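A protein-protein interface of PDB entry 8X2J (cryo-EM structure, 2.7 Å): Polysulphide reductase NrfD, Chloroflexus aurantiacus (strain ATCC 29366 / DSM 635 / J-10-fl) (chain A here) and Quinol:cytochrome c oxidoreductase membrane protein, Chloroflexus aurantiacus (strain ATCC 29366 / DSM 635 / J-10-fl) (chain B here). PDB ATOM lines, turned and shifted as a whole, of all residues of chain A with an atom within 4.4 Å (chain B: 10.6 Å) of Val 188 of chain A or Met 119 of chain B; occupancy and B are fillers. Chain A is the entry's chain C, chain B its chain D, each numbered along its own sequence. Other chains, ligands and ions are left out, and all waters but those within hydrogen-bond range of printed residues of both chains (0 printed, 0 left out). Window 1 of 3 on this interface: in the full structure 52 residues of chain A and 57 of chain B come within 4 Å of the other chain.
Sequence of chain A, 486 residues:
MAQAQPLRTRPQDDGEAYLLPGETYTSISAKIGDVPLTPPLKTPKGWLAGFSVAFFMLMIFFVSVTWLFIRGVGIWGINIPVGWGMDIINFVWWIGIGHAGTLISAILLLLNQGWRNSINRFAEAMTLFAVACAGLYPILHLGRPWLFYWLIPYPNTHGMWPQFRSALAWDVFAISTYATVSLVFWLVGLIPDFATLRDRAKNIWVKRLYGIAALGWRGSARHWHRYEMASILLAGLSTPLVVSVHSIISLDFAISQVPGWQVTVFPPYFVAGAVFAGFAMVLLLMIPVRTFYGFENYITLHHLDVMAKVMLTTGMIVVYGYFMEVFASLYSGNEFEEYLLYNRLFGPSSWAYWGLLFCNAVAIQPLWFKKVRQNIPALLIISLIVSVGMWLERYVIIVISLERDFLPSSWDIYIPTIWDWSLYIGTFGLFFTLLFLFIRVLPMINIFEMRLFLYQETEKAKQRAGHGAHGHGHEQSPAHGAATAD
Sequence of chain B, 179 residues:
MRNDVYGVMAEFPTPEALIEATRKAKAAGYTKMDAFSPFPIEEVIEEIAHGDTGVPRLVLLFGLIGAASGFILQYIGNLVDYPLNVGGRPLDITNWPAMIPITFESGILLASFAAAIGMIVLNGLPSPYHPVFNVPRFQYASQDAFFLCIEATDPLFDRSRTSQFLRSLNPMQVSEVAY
Val 184 of chain A touches just one residue of chain B: Ala 116 (3.6 Å). Printed residues of chain B within 4 Å of Val 188 of chain A: Met 119 (3.99 Å). Ile 191 of chain A touches none of the printed residues of chain B. Of the printed residues of chain B, Arg 226 of chain A touches Thr 53 (3.2 Å), Val 55 (3.96 Å), Met 119 (3.3 Å), Leu 122 (3.6 Å) and Asn 123 (3.5 Å). Of the printed residues of chain B, Tyr 227 of chain A touches Met 119. Of the printed residues of chain B, Ala 230 of chain A touches Met 119 (3.7 Å). Printed residues of chain A within 4 Å of Val 55 of chain B: Arg 226. Of the printed residues of chain A, Ala 116 of chain B touches Val 184. Of the printed residues of chain A, Met 119 of chain B touches Val 188, Arg 226, Tyr 227 and Ala 230. Of the printed residues of chain A, Leu 122 of chain B touches Arg 226 (3.6 Å). Pro 126 of chain B touches none of the printed residues of chain A. The nearest printed residue of chain A that does not touch Met 119 of chain B is Ile 191 of chain A (6.1 Å).
The guanidinium group of Arg 226 of chain A lies within hydrogen-bond range of the backbone carbonyl oxygen of Thr 53 of chain B (3.2 Å).
CB of Ala 116 of chain B touches CG1 of Val 184 of chain A (3.6 Å). CG1 of Val 188 of chain A touches CE of Met 119 of chain B, 3.99 Å away. Arg 226 of chain A touches Val 55 of chain B (CG to CG2, 3.96 Å). CG of Met 119 of chain B touches O of Arg 226 of chain A, at 3.3 Å. Arg 226 of chain A touches Leu 122 of chain B (CZ to O, 3.6 Å). Asn 123 of chain B touches Arg 226 of chain A (N to CD, 3.5 Å). CE of Met 119 of chain B touches CD1 of Tyr 227 of chain A (3.7 Å). Ala 230 of chain A touches Met 119 of chain B.
Of the 26 printed residues of chain B, 6 touch a printed residue of chain A. Of the 12 printed residues of chain A, 5 touch a printed residue of chain B. Printed residues of chain A that touch a printed residue of chain B: Val 184, Val 188, Arg 226, Tyr 227 and Ala 230. Hydrophobic or aromatic side chains of chain A within 4 Å of the printed part of chain B: Val 184, Val 188, Tyr 227 and Ala 230. Among the printed residues, 9 pairs touch across the chains.
OG1 of Thr 53 of chain B is in hydrogen-bond range of N of Val 55 of chain B. OD1 of Asn 123 of chain B sits close to O of Met 119 of chain B. The backbone carbonyl oxygen (O) of Ile 120 of chain B lies close to the side-chain amide oxygen (OD1) of Asn 123 of chain B, at 2.6 Å. OD1 of Asn 123 of chain B is in hydrogen-bond range of N of Leu 125 of chain B, at 2.8 Å.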
ATOM      1  N   VAL A 184     -17.820  18.956  11.131  1.00  0.00           N
ATOM      2  CA  VAL A 184     -16.508  18.440  10.746  1.00  0.00           C
ATOM      3  C   VAL A 184     -16.441  18.180   9.244  1.00  0.00           C
ATOM      4  O   VAL A 184     -15.482  18.582   8.573  1.00  0.00           O
ATOM      5  CB  VAL A 184     -16.188  17.179  11.572  1.00  0.00           C
ATOM      6  CG1 VAL A 184     -15.154  16.334  10.900  1.00  0.00           C
ATOM      7  CG2 VAL A 184     -15.672  17.579  12.944  1.00  0.00           C
ATOM      8  N   PHE A 185     -17.472  17.541   8.688  1.00  0.00           N
ATOM      9  CA  PHE A 185     -17.500  17.249   7.259  1.00  0.00           C
ATOM     10  C   PHE A 185     -17.653  18.518   6.426  1.00  0.00           C
ATOM     11  O   PHE A 185     -17.062  18.619   5.345  1.00  0.00           O
ATOM     12  CB  PHE A 185     -18.623  16.251   6.968  1.00  0.00           C
ATOM     13  CG  PHE A 185     -18.519  15.584   5.627  1.00  0.00           C
ATOM     14  CD1 PHE A 185     -17.285  15.374   5.032  1.00  0.00           C
ATOM     15  CD2 PHE A 185     -19.654  15.128   4.980  1.00  0.00           C
ATOM     16  CE1 PHE A 185     -17.189  14.753   3.802  1.00  0.00           C
ATOM     17  CE2 PHE A 185     -19.563  14.501   3.753  1.00  0.00           C
ATOM     18  CZ  PHE A 185     -18.329  14.314   3.165  1.00  0.00           C
ATOM     19  N   TRP A 186     -18.400  19.505   6.931  1.00  0.00           N
ATOM     20  CA  TRP A 186     -18.513  20.793   6.252  1.00  0.00           C
ATOM     21  C   TRP A 186     -17.184  21.545   6.243  1.00  0.00           C
ATOM     22  O   TRP A 186     -16.804  22.132   5.226  1.00  0.00           O
ATOM     23  CB  TRP A 186     -19.600  21.619   6.933  1.00  0.00           C
ATOM     24  CG  TRP A 186     -20.061  22.825   6.187  1.00  0.00           C
ATOM     25  CD1 TRP A 186     -20.659  22.858   4.962  1.00  0.00           C
ATOM     26  CD2 TRP A 186     -19.977  24.183   6.628  1.00  0.00           C
ATOM     27  NE1 TRP A 186     -20.949  24.151   4.612  1.00  0.00           N
ATOM     28  CE2 TRP A 186     -20.538  24.985   5.619  1.00  0.00           C
ATOM     29  CE3 TRP A 186     -19.471  24.799   7.777  1.00  0.00           C
ATOM     30  CZ2 TRP A 186     -20.613  26.368   5.726  1.00  0.00           C
ATOM     31  CZ3 TRP A 186     -19.550  26.168   7.882  1.00  0.00           C
ATOM     32  CH2 TRP A 186     -20.117  26.938   6.863  1.00  0.00           C
ATOM     33  N   LEU A 187     -16.452  21.520   7.360  1.00  0.00           N
ATOM     34  CA  LEU A 187     -15.155  22.191   7.410  1.00  0.00           C
ATOM     35  C   LEU A 187     -14.116  21.473   6.551  1.00  0.00           C
ATOM     36  O   LEU A 187     -13.257  22.119   5.934  1.00  0.00           O
ATOM     37  CB  LEU A 187     -14.687  22.300   8.859  1.00  0.00           C
ATOM     38  CG  LEU A 187     -15.395  23.371   9.692  1.00  0.00           C
ATOM     39  CD1 LEU A 187     -15.140  23.155  11.172  1.00  0.00           C
ATOM     40  CD2 LEU A 187     -14.948  24.757   9.270  1.00  0.00           C
ATOM     41  N   VAL A 188     -14.189  20.139   6.494  1.00  0.00           N
ATOM     42  CA  VAL A 188     -13.315  19.362   5.616  1.00  0.00           C
ATOM     43  C   VAL A 188     -13.609  19.686   4.155  1.00  0.00           C
ATOM     44  O   VAL A 188     -12.690  19.901   3.355  1.00  0.00           O
ATOM     45  CB  VAL A 188     -13.462  17.859   5.927  1.00  0.00           C
ATOM     46  CG1 VAL A 188     -13.011  16.989   4.759  1.00  0.00           C
ATOM     47  CG2 VAL A 188     -12.669  17.506   7.174  1.00  0.00           C
ATOM     48  N   GLY A 189     -14.889  19.788   3.798  1.00  0.00           N
ATOM     49  CA  GLY A 189     -15.258  20.250   2.472  1.00  0.00           C
ATOM     50  C   GLY A 189     -14.982  21.717   2.211  1.00  0.00           C
ATOM     51  O   GLY A 189     -15.067  22.145   1.058  1.00  0.00           O
ATOM     52  N   LEU A 190     -14.701  22.500   3.249  1.00  0.00           N
ATOM     53  CA  LEU A 190     -14.354  23.904   3.077  1.00  0.00           C
ATOM     54  C   LEU A 190     -12.856  24.179   3.018  1.00  0.00           C
ATOM     55  O   LEU A 190     -12.480  25.277   2.598  1.00  0.00           O
ATOM     56  CB  LEU A 190     -14.949  24.734   4.216  1.00  0.00           C
ATOM     57  CG  LEU A 190     -16.361  25.297   4.101  1.00  0.00           C
ATOM     58  CD1 LEU A 190     -16.838  25.711   5.465  1.00  0.00           C
ATOM     59  CD2 LEU A 190     -16.356  26.494   3.179  1.00  0.00           C
ATOM     60  N   ILE A 191     -12.010  23.232   3.459  1.00  0.00           N
ATOM     61  CA  ILE A 191     -10.571  23.520   3.613  1.00  0.00           C
ATOM     62  C   ILE A 191      -9.861  23.899   2.306  1.00  0.00           C
ATOM     63  O   ILE A 191      -9.140  24.911   2.299  1.00  0.00           O
ATOM     64  CB  ILE A 191      -9.886  22.377   4.386  1.00  0.00           C
ATOM     65  CG1 ILE A 191     -10.016  22.585   5.892  1.00  0.00           C
ATOM     66  CG2 ILE A 191      -8.407  22.244   4.028  1.00  0.00           C
ATOM     67  CD1 ILE A 191      -9.615  21.376   6.699  1.00  0.00           C
ATOM     68  N   PRO A 192     -10.044  23.197   1.170  1.00  0.00           N
ATOM     69  CA  PRO A 192      -9.476  23.760  -0.071  1.00  0.00           C
ATOM     70  C   PRO A 192     -10.272  24.922  -0.655  1.00  0.00           C
ATOM     71  O   PRO A 192      -9.694  25.714  -1.408  1.00  0.00           O
ATOM     72  CB  PRO A 192      -9.418  22.564  -1.029  1.00  0.00           C
ATOM     73  CG  PRO A 192     -10.280  21.587  -0.502  1.00  0.00           C
ATOM     74  CD  PRO A 192     -10.465  21.796   0.946  1.00  0.00           C
ATOM     75  N   ARG A 226      -5.527  11.174   0.413  1.00  0.00           N
ATOM     76  CA  ARG A 226      -6.027  11.086   1.779  1.00  0.00           C
ATOM     77  C   ARG A 226      -7.308  11.886   1.960  1.00  0.00           C
ATOM     78  O   ARG A 226      -8.192  11.466   2.713  1.00  0.00           O
ATOM     79  CB  ARG A 226      -4.960  11.573   2.756  1.00  0.00           C
ATOM     80  CG  ARG A 226      -4.150  10.465   3.381  1.00  0.00           C
ATOM     81  CD  ARG A 226      -2.957  11.016   4.117  1.00  0.00           C
ATOM     82  NE  ARG A 226      -1.800  11.181   3.247  1.00  0.00           N
ATOM     83  CZ  ARG A 226      -0.735  10.391   3.267  1.00  0.00           C
ATOM     84  NH1 ARG A 226      -0.655   9.361   4.092  1.00  0.00           N
ATOM     85  NH2 ARG A 226       0.275  10.643   2.439  1.00  0.00           N
ATOM     86  N   TYR A 227      -7.425  13.021   1.264  1.00  0.00           N
ATOM     87  CA  TYR A 227      -8.643  13.823   1.313  1.00  0.00           C
ATOM     88  C   TYR A 227      -9.833  13.078   0.727  1.00  0.00           C
ATOM     89  O   TYR A 227     -10.926  13.096   1.303  1.00  0.00           O
ATOM     90  CB  TYR A 227      -8.422  15.133   0.562  1.00  0.00           C
ATOM     91  CG  TYR A 227      -9.521  16.146   0.742  1.00  0.00           C
ATOM     92  CD1 TYR A 227      -9.535  16.990   1.842  1.00  0.00           C
ATOM     93  CD2 TYR A 227     -10.543  16.264  -0.195  1.00  0.00           C
ATOM     94  CE1 TYR A 227     -10.536  17.918   2.009  1.00  0.00           C
ATOM     95  CE2 TYR A 227     -11.549  17.186  -0.033  1.00  0.00           C
ATOM     96  CZ  TYR A 227     -11.539  18.009   1.069  1.00  0.00           C
ATOM     97  OH  TYR A 227     -12.537  18.930   1.229  1.00  0.00           O
ATOM     98  N   ALA A 230     -10.770  10.218   3.090  1.00  0.00           N
ATOM     99  CA  ALA A 230     -11.459  10.732   4.268  1.00  0.00           C
ATOM    100  C   ALA A 230     -12.869  11.193   3.938  1.00  0.00           C
ATOM    101  O   ALA A 230     -13.785  10.994   4.737  1.00  0.00           O
ATOM    102  CB  ALA A 230     -10.667  11.878   4.883  1.00  0.00           C
ATOM    103  N   THR B  53      -3.839   4.920   2.135  1.00  0.00           N
ATOM    104  CA  THR B  53      -3.803   6.265   2.697  1.00  0.00           C
ATOM    105  C   THR B  53      -3.524   6.251   4.195  1.00  0.00           C
ATOM    106  O   THR B  53      -2.931   7.199   4.722  1.00  0.00           O
ATOM    107  CB  THR B  53      -5.123   6.983   2.416  1.00  0.00           C
ATOM    108  OG1 THR B  53      -6.151   6.429   3.243  1.00  0.00           O
ATOM    109  CG2 THR B  53      -5.517   6.815   0.963  1.00  0.00           C
ATOM    110  N   GLY B  54      -3.931   5.193   4.893  1.00  0.00           N
ATOM    111  CA  GLY B  54      -3.815   5.124   6.332  1.00  0.00           C
ATOM    112  C   GLY B  54      -5.020   5.639   7.085  1.00  0.00           C
ATOM    113  O   GLY B  54      -5.093   5.453   8.306  1.00  0.00           O
ATOM    114  N   VAL B  55      -5.951   6.299   6.396  1.00  0.00           N
ATOM    115  CA  VAL B  55      -7.202   6.730   7.031  1.00  0.00           C
ATOM    116  C   VAL B  55      -8.096   5.576   7.502  1.00  0.00           C
ATOM    117  O   VAL B  55      -8.522   5.605   8.669  1.00  0.00           O
ATOM    118  CB  VAL B  55      -7.939   7.721   6.128  1.00  0.00           C
ATOM    119  CG1 VAL B  55      -9.039   8.428   6.897  1.00  0.00           C
ATOM    120  CG2 VAL B  55      -6.970   8.739   5.556  1.00  0.00           C
ATOM    121  N   PRO B  56      -8.453   4.565   6.665  1.00  0.00           N
ATOM    122  CA  PRO B  56      -9.495   3.611   7.106  1.00  0.00           C
ATOM    123  C   PRO B  56      -9.097   2.713   8.263  1.00  0.00           C
ATOM    124  O   PRO B  56      -9.988   2.257   8.988  1.00  0.00           O
ATOM    125  CB  PRO B  56      -9.780   2.779   5.846  1.00  0.00           C
ATOM    126  CG  PRO B  56      -9.213   3.529   4.739  1.00  0.00           C
ATOM    127  CD  PRO B  56      -8.017   4.180   5.305  1.00  0.00           C
ATOM    128  N   ARG B  57      -7.802   2.461   8.469  1.00  0.00           N
ATOM    129  CA  ARG B  57      -7.367   1.713   9.645  1.00  0.00           C
ATOM    130  C   ARG B  57      -7.671   2.477  10.929  1.00  0.00           C
ATOM    131  O   ARG B  57      -8.190   1.904  11.896  1.00  0.00           O
ATOM    132  CB  ARG B  57      -5.874   1.411   9.538  1.00  0.00           C
ATOM    133  CG  ARG B  57      -5.336   0.503  10.623  1.00  0.00           C
ATOM    134  CD  ARG B  57      -3.916   0.066  10.304  1.00  0.00           C
ATOM    135  NE  ARG B  57      -3.221   1.039   9.470  1.00  0.00           N
ATOM    136  CZ  ARG B  57      -2.008   0.862   8.967  1.00  0.00           C
ATOM    137  NH1 ARG B  57      -1.319  -0.244   9.198  1.00  0.00           N
ATOM    138  NH2 ARG B  57      -1.471   1.818   8.215  1.00  0.00           N
ATOM    139  N   LEU B  58      -7.387   3.784  10.939  1.00  0.00           N
ATOM    140  CA  LEU B  58      -7.717   4.622  12.086  1.00  0.00           C
ATOM    141  C   LEU B  58      -9.223   4.760  12.261  1.00  0.00           C
ATOM    142  O   LEU B  58      -9.717   4.797  13.397  1.00  0.00           O
ATOM    143  CB  LEU B  58      -7.073   5.998  11.930  1.00  0.00           C
ATOM    144  CG  LEU B  58      -5.547   6.031  11.945  1.00  0.00           C
ATOM    145  CD1 LEU B  58      -5.051   7.434  11.663  1.00  0.00           C
ATOM    146  CD2 LEU B  58      -5.019   5.529  13.276  1.00  0.00           C
ATOM    147  N   VAL B  59      -9.964   4.833  11.148  1.00  0.00           N
ATOM    148  CA  VAL B  59     -11.423   4.933  11.212  1.00  0.00           C
ATOM    149  C   VAL B  59     -12.019   3.677  11.840  1.00  0.00           C
ATOM    150  O   VAL B  59     -12.868   3.758  12.735  1.00  0.00           O
ATOM    151  CB  VAL B  59     -12.009   5.195   9.813  1.00  0.00           C
ATOM    152  CG1 VAL B  59     -13.524   5.126   9.841  1.00  0.00           C
ATOM    153  CG2 VAL B  59     -11.582   6.542   9.317  1.00  0.00           C
ATOM    154  N   PHE B  62     -10.902   3.521  15.770  1.00  0.00           N
ATOM    155  CA  PHE B  62     -11.654   4.392  16.659  1.00  0.00           C
ATOM    156  C   PHE B  62     -13.157   4.170  16.581  1.00  0.00           C
ATOM    157  O   PHE B  62     -13.852   4.492  17.544  1.00  0.00           O
ATOM    158  CB  PHE B  62     -11.328   5.856  16.384  1.00  0.00           C
ATOM    159  CG  PHE B  62     -10.011   6.294  16.949  1.00  0.00           C
ATOM    160  CD1 PHE B  62      -9.928   6.782  18.242  1.00  0.00           C
ATOM    161  CD2 PHE B  62      -8.854   6.209  16.192  1.00  0.00           C
ATOM    162  CE1 PHE B  62      -8.715   7.180  18.770  1.00  0.00           C
ATOM    163  CE2 PHE B  62      -7.639   6.607  16.710  1.00  0.00           C
ATOM    164  CZ  PHE B  62      -7.570   7.093  18.001  1.00  0.00           C
ATOM    165  N   LEU B 110     -16.518   8.779  17.155  1.00  0.00           N
ATOM    166  CA  LEU B 110     -15.073   8.589  17.205  1.00  0.00           C
ATOM    167  C   LEU B 110     -14.504   8.132  15.865  1.00  0.00           C
ATOM    168  O   LEU B 110     -13.353   8.450  15.556  1.00  0.00           O
ATOM    169  CB  LEU B 110     -14.689   7.631  18.332  1.00  0.00           C
ATOM    170  CG  LEU B 110     -14.827   8.269  19.719  1.00  0.00           C
ATOM    171  CD1 LEU B 110     -14.408   7.318  20.815  1.00  0.00           C
ATOM    172  CD2 LEU B 110     -14.026   9.559  19.808  1.00  0.00           C
ATOM    173  N   ALA B 111     -15.297   7.454  15.028  1.00  0.00           N
ATOM    174  CA  ALA B 111     -14.811   7.088  13.701  1.00  0.00           C
ATOM    175  C   ALA B 111     -14.693   8.306  12.790  1.00  0.00           C
ATOM    176  O   ALA B 111     -13.752   8.403  11.996  1.00  0.00           O
ATOM    177  CB  ALA B 111     -15.726   6.037  13.081  1.00  0.00           C
ATOM    178  N   SER B 112     -15.626   9.256  12.900  1.00  0.00           N
ATOM    179  CA  SER B 112     -15.539  10.473  12.099  1.00  0.00           C
ATOM    180  C   SER B 112     -14.429  11.391  12.597  1.00  0.00           C
ATOM    181  O   SER B 112     -13.766  12.065  11.793  1.00  0.00           O
ATOM    182  CB  SER B 112     -16.878  11.197  12.113  1.00  0.00           C
ATOM    183  OG  SER B 112     -17.925  10.334  11.714  1.00  0.00           O
ATOM    184  N   PHE B 113     -14.216  11.430  13.919  1.00  0.00           N
ATOM    185  CA  PHE B 113     -13.051  12.119  14.467  1.00  0.00           C
ATOM    186  C   PHE B 113     -11.759  11.491  13.963  1.00  0.00           C
ATOM    187  O   PHE B 113     -10.799  12.203  13.646  1.00  0.00           O
ATOM    188  CB  PHE B 113     -13.080  12.086  15.994  1.00  0.00           C
ATOM    189  CG  PHE B 113     -13.980  13.112  16.613  1.00  0.00           C
ATOM    190  CD1 PHE B 113     -14.511  14.147  15.858  1.00  0.00           C
ATOM    191  CD2 PHE B 113     -14.283  13.047  17.964  1.00  0.00           C
ATOM    192  CE1 PHE B 113     -15.336  15.088  16.438  1.00  0.00           C
ATOM    193  CE2 PHE B 113     -15.104  13.984  18.550  1.00  0.00           C
ATOM    194  CZ  PHE B 113     -15.630  15.005  17.787  1.00  0.00           C
ATOM    195  N   ALA B 114     -11.724  10.156  13.886  1.00  0.00           N
ATOM    196  CA  ALA B 114     -10.569   9.458  13.339  1.00  0.00           C
ATOM    197  C   ALA B 114     -10.344   9.814  11.881  1.00  0.00           C
ATOM    198  O   ALA B 114      -9.210  10.080  11.486  1.00  0.00           O
ATOM    199  CB  ALA B 114     -10.747   7.954  13.482  1.00  0.00           C
ATOM    200  N   ALA B 115     -11.420   9.870  11.087  1.00  0.00           N
ATOM    201  CA  ALA B 115     -11.313  10.217   9.670  1.00  0.00           C
ATOM    202  C   ALA B 115     -10.737  11.613   9.480  1.00  0.00           C
ATOM    203  O   ALA B 115      -9.724  11.786   8.789  1.00  0.00           O
ATOM    204  CB  ALA B 115     -12.682  10.110   8.999  1.00  0.00           C
ATOM    205  N   ALA B 116     -11.312  12.600  10.176  1.00  0.00           N
ATOM    206  CA  ALA B 116     -10.863  13.984  10.050  1.00  0.00           C
ATOM    207  C   ALA B 116      -9.442  14.174  10.567  1.00  0.00           C
ATOM    208  O   ALA B 116      -8.551  14.577   9.809  1.00  0.00           O
ATOM    209  CB  ALA B 116     -11.816  14.909  10.796  1.00  0.00           C
ATOM    210  N   ILE B 117      -9.214  13.879  11.853  1.00  0.00           N
ATOM    211  CA  ILE B 117      -7.924  14.153  12.479  1.00  0.00           C
ATOM    212  C   ILE B 117      -6.833  13.268  11.886  1.00  0.00           C
ATOM    213  O   ILE B 117      -5.695  13.715  11.700  1.00  0.00           O
ATOM    214  CB  ILE B 117      -8.034  13.995  14.009  1.00  0.00           C
ATOM    215  CG1 ILE B 117      -9.164  14.871  14.556  1.00  0.00           C
ATOM    216  CG2 ILE B 117      -6.737  14.370  14.705  1.00  0.00           C
ATOM    217  CD1 ILE B 117      -8.991  16.343  14.274  1.00  0.00           C
ATOM    218  N   GLY B 118      -7.166  12.022  11.534  1.00  0.00           N
ATOM    219  CA  GLY B 118      -6.200  11.150  10.900  1.00  0.00           C
ATOM    220  C   GLY B 118      -5.803  11.612   9.516  1.00  0.00           C
ATOM    221  O   GLY B 118      -4.629  11.544   9.164  1.00  0.00           O
ATOM    222  N   MET B 119      -6.760  12.122   8.725  1.00  0.00           N
ATOM    223  CA  MET B 119      -6.403  12.683   7.424  1.00  0.00           C
ATOM    224  C   MET B 119      -5.521  13.914   7.575  1.00  0.00           C
ATOM    225  O   MET B 119      -4.477  14.015   6.916  1.00  0.00           O
ATOM    226  CB  MET B 119      -7.656  13.034   6.633  1.00  0.00           C
ATOM    227  CG  MET B 119      -7.364  13.521   5.223  1.00  0.00           C
ATOM    228  SD  MET B 119      -7.586  15.295   5.005  1.00  0.00           S
ATOM    229  CE  MET B 119      -9.363  15.432   5.161  1.00  0.00           C
ATOM    230  N   ILE B 120      -5.905  14.827   8.481  1.00  0.00           N
ATOM    231  CA  ILE B 120      -5.187  16.089   8.671  1.00  0.00           C
ATOM    232  C   ILE B 120      -3.762  15.836   9.159  1.00  0.00           C
ATOM    233  O   ILE B 120      -2.806  16.446   8.665  1.00  0.00           O
ATOM    234  CB  ILE B 120      -5.967  17.005   9.641  1.00  0.00           C
ATOM    235  CG1 ILE B 120      -7.324  17.423   9.064  1.00  0.00           C
ATOM    236  CG2 ILE B 120      -5.188  18.254   9.978  1.00  0.00           C
ATOM    237  CD1 ILE B 120      -7.302  17.884   7.646  1.00  0.00           C
ATOM    238  N   VAL B 121      -3.594  14.912  10.108  1.00  0.00           N
ATOM    239  CA  VAL B 121      -2.263  14.583  10.610  1.00  0.00           C
ATOM    240  C   VAL B 121      -1.467  13.794   9.572  1.00  0.00           C
ATOM    241  O   VAL B 121      -0.283  14.073   9.340  1.00  0.00           O
ATOM    242  CB  VAL B 121      -2.387  13.829  11.949  1.00  0.00           C
ATOM    243  CG1 VAL B 121      -1.069  13.187  12.355  1.00  0.00           C
ATOM    244  CG2 VAL B 121      -2.863  14.773  13.037  1.00  0.00           C
ATOM    245  N   LEU B 122      -2.107  12.830   8.901  1.00  0.00           N
ATOM    246  CA  LEU B 122      -1.389  11.884   8.056  1.00  0.00           C
ATOM    247  C   LEU B 122      -0.893  12.516   6.765  1.00  0.00           C
ATOM    248  O   LEU B 122       0.152  12.104   6.251  1.00  0.00           O
ATOM    249  CB  LEU B 122      -2.283  10.684   7.750  1.00  0.00           C
ATOM    250  CG  LEU B 122      -2.127   9.470   8.665  1.00  0.00           C
ATOM    251  CD1 LEU B 122      -3.226   8.472   8.382  1.00  0.00           C
ATOM    252  CD2 LEU B 122      -0.768   8.835   8.491  1.00  0.00           C
ATOM    253  N   ASN B 123      -1.642  13.484   6.231  1.00  0.00           N
ATOM    254  CA  ASN B 123      -1.172  14.199   5.015  1.00  0.00           C
ATOM    255  C   ASN B 123      -0.197  15.296   5.448  1.00  0.00           C
ATOM    256  O   ASN B 123       0.417  15.917   4.564  1.00  0.00           O
ATOM    257  CB  ASN B 123      -2.333  14.749   4.180  1.00  0.00           C
ATOM    258  CG  ASN B 123      -3.107  15.845   4.880  1.00  0.00           C
ATOM    259  OD1 ASN B 123      -2.886  16.112   6.058  1.00  0.00           O
ATOM    260  ND2 ASN B 123      -4.019  16.483   4.165  1.00  0.00           N
ATOM    261  N   GLY B 124      -0.050  15.507   6.759  1.00  0.00           N
ATOM    262  CA  GLY B 124       0.821  16.588   7.259  1.00  0.00           C
ATOM    263  C   GLY B 124       0.251  17.951   6.908  1.00  0.00           C
ATOM    264  O   GLY B 124       1.046  18.885   6.686  1.00  0.00           O
ATOM    265  N   LEU B 125      -1.081  18.061   6.860  1.00  0.00           N
ATOM    266  CA  LEU B 125      -1.743  19.346   6.501  1.00  0.00           C
ATOM    267  C   LEU B 125      -1.389  20.445   7.514  1.00  0.00           C
ATOM    268  O   LEU B 125      -1.220  21.592   7.067  1.00  0.00           O
ATOM    269  CB  LEU B 125      -3.259  19.138   6.431  1.00  0.00           C
ATOM    270  CG  LEU B 125      -4.047  20.344   5.920  1.00  0.00           C
ATOM    271  CD1 LEU B 125      -3.486  20.828   4.592  1.00  0.00           C
ATOM    272  CD2 LEU B 125      -5.524  20.011   5.779  1.00  0.00           C
ATOM    273  N   PRO B 126      -1.282  20.179   8.839  1.00  0.00           N
ATOM    274  CA  PRO B 126      -1.031  21.242   9.826  1.00  0.00           C
ATOM    275  C   PRO B 126       0.323  21.934   9.616  1.00  0.00           C
ATOM    276  O   PRO B 126       1.051  22.088  10.582  1.00  0.00           O
ATOM    277  CB  PRO B 126      -1.018  20.507  11.176  1.00  0.00           C
ATOM    278  CG  PRO B 126      -1.792  19.237  10.915  1.00  0.00           C
ATOM    279  CD  PRO B 126      -1.442  18.876   9.488  1.00  0.00           C
ATOM    280  N   SER B 127       0.625  22.333   8.379  1.00  0.00           N
ATOM    281  CA  SER B 127       1.883  23.063   8.079  1.00  0.00           C
ATOM    282  C   SER B 127       1.548  24.265   7.193  1.00  0.00           C
ATOM    283  O   SER B 127       1.933  24.251   6.006  1.00  0.00           O
ATOM    284  CB  SER B 127       2.889  22.157   7.423  1.00  0.00           C
ATOM    285  OG  SER B 127       2.341  21.557   6.258  1.00  0.00           O
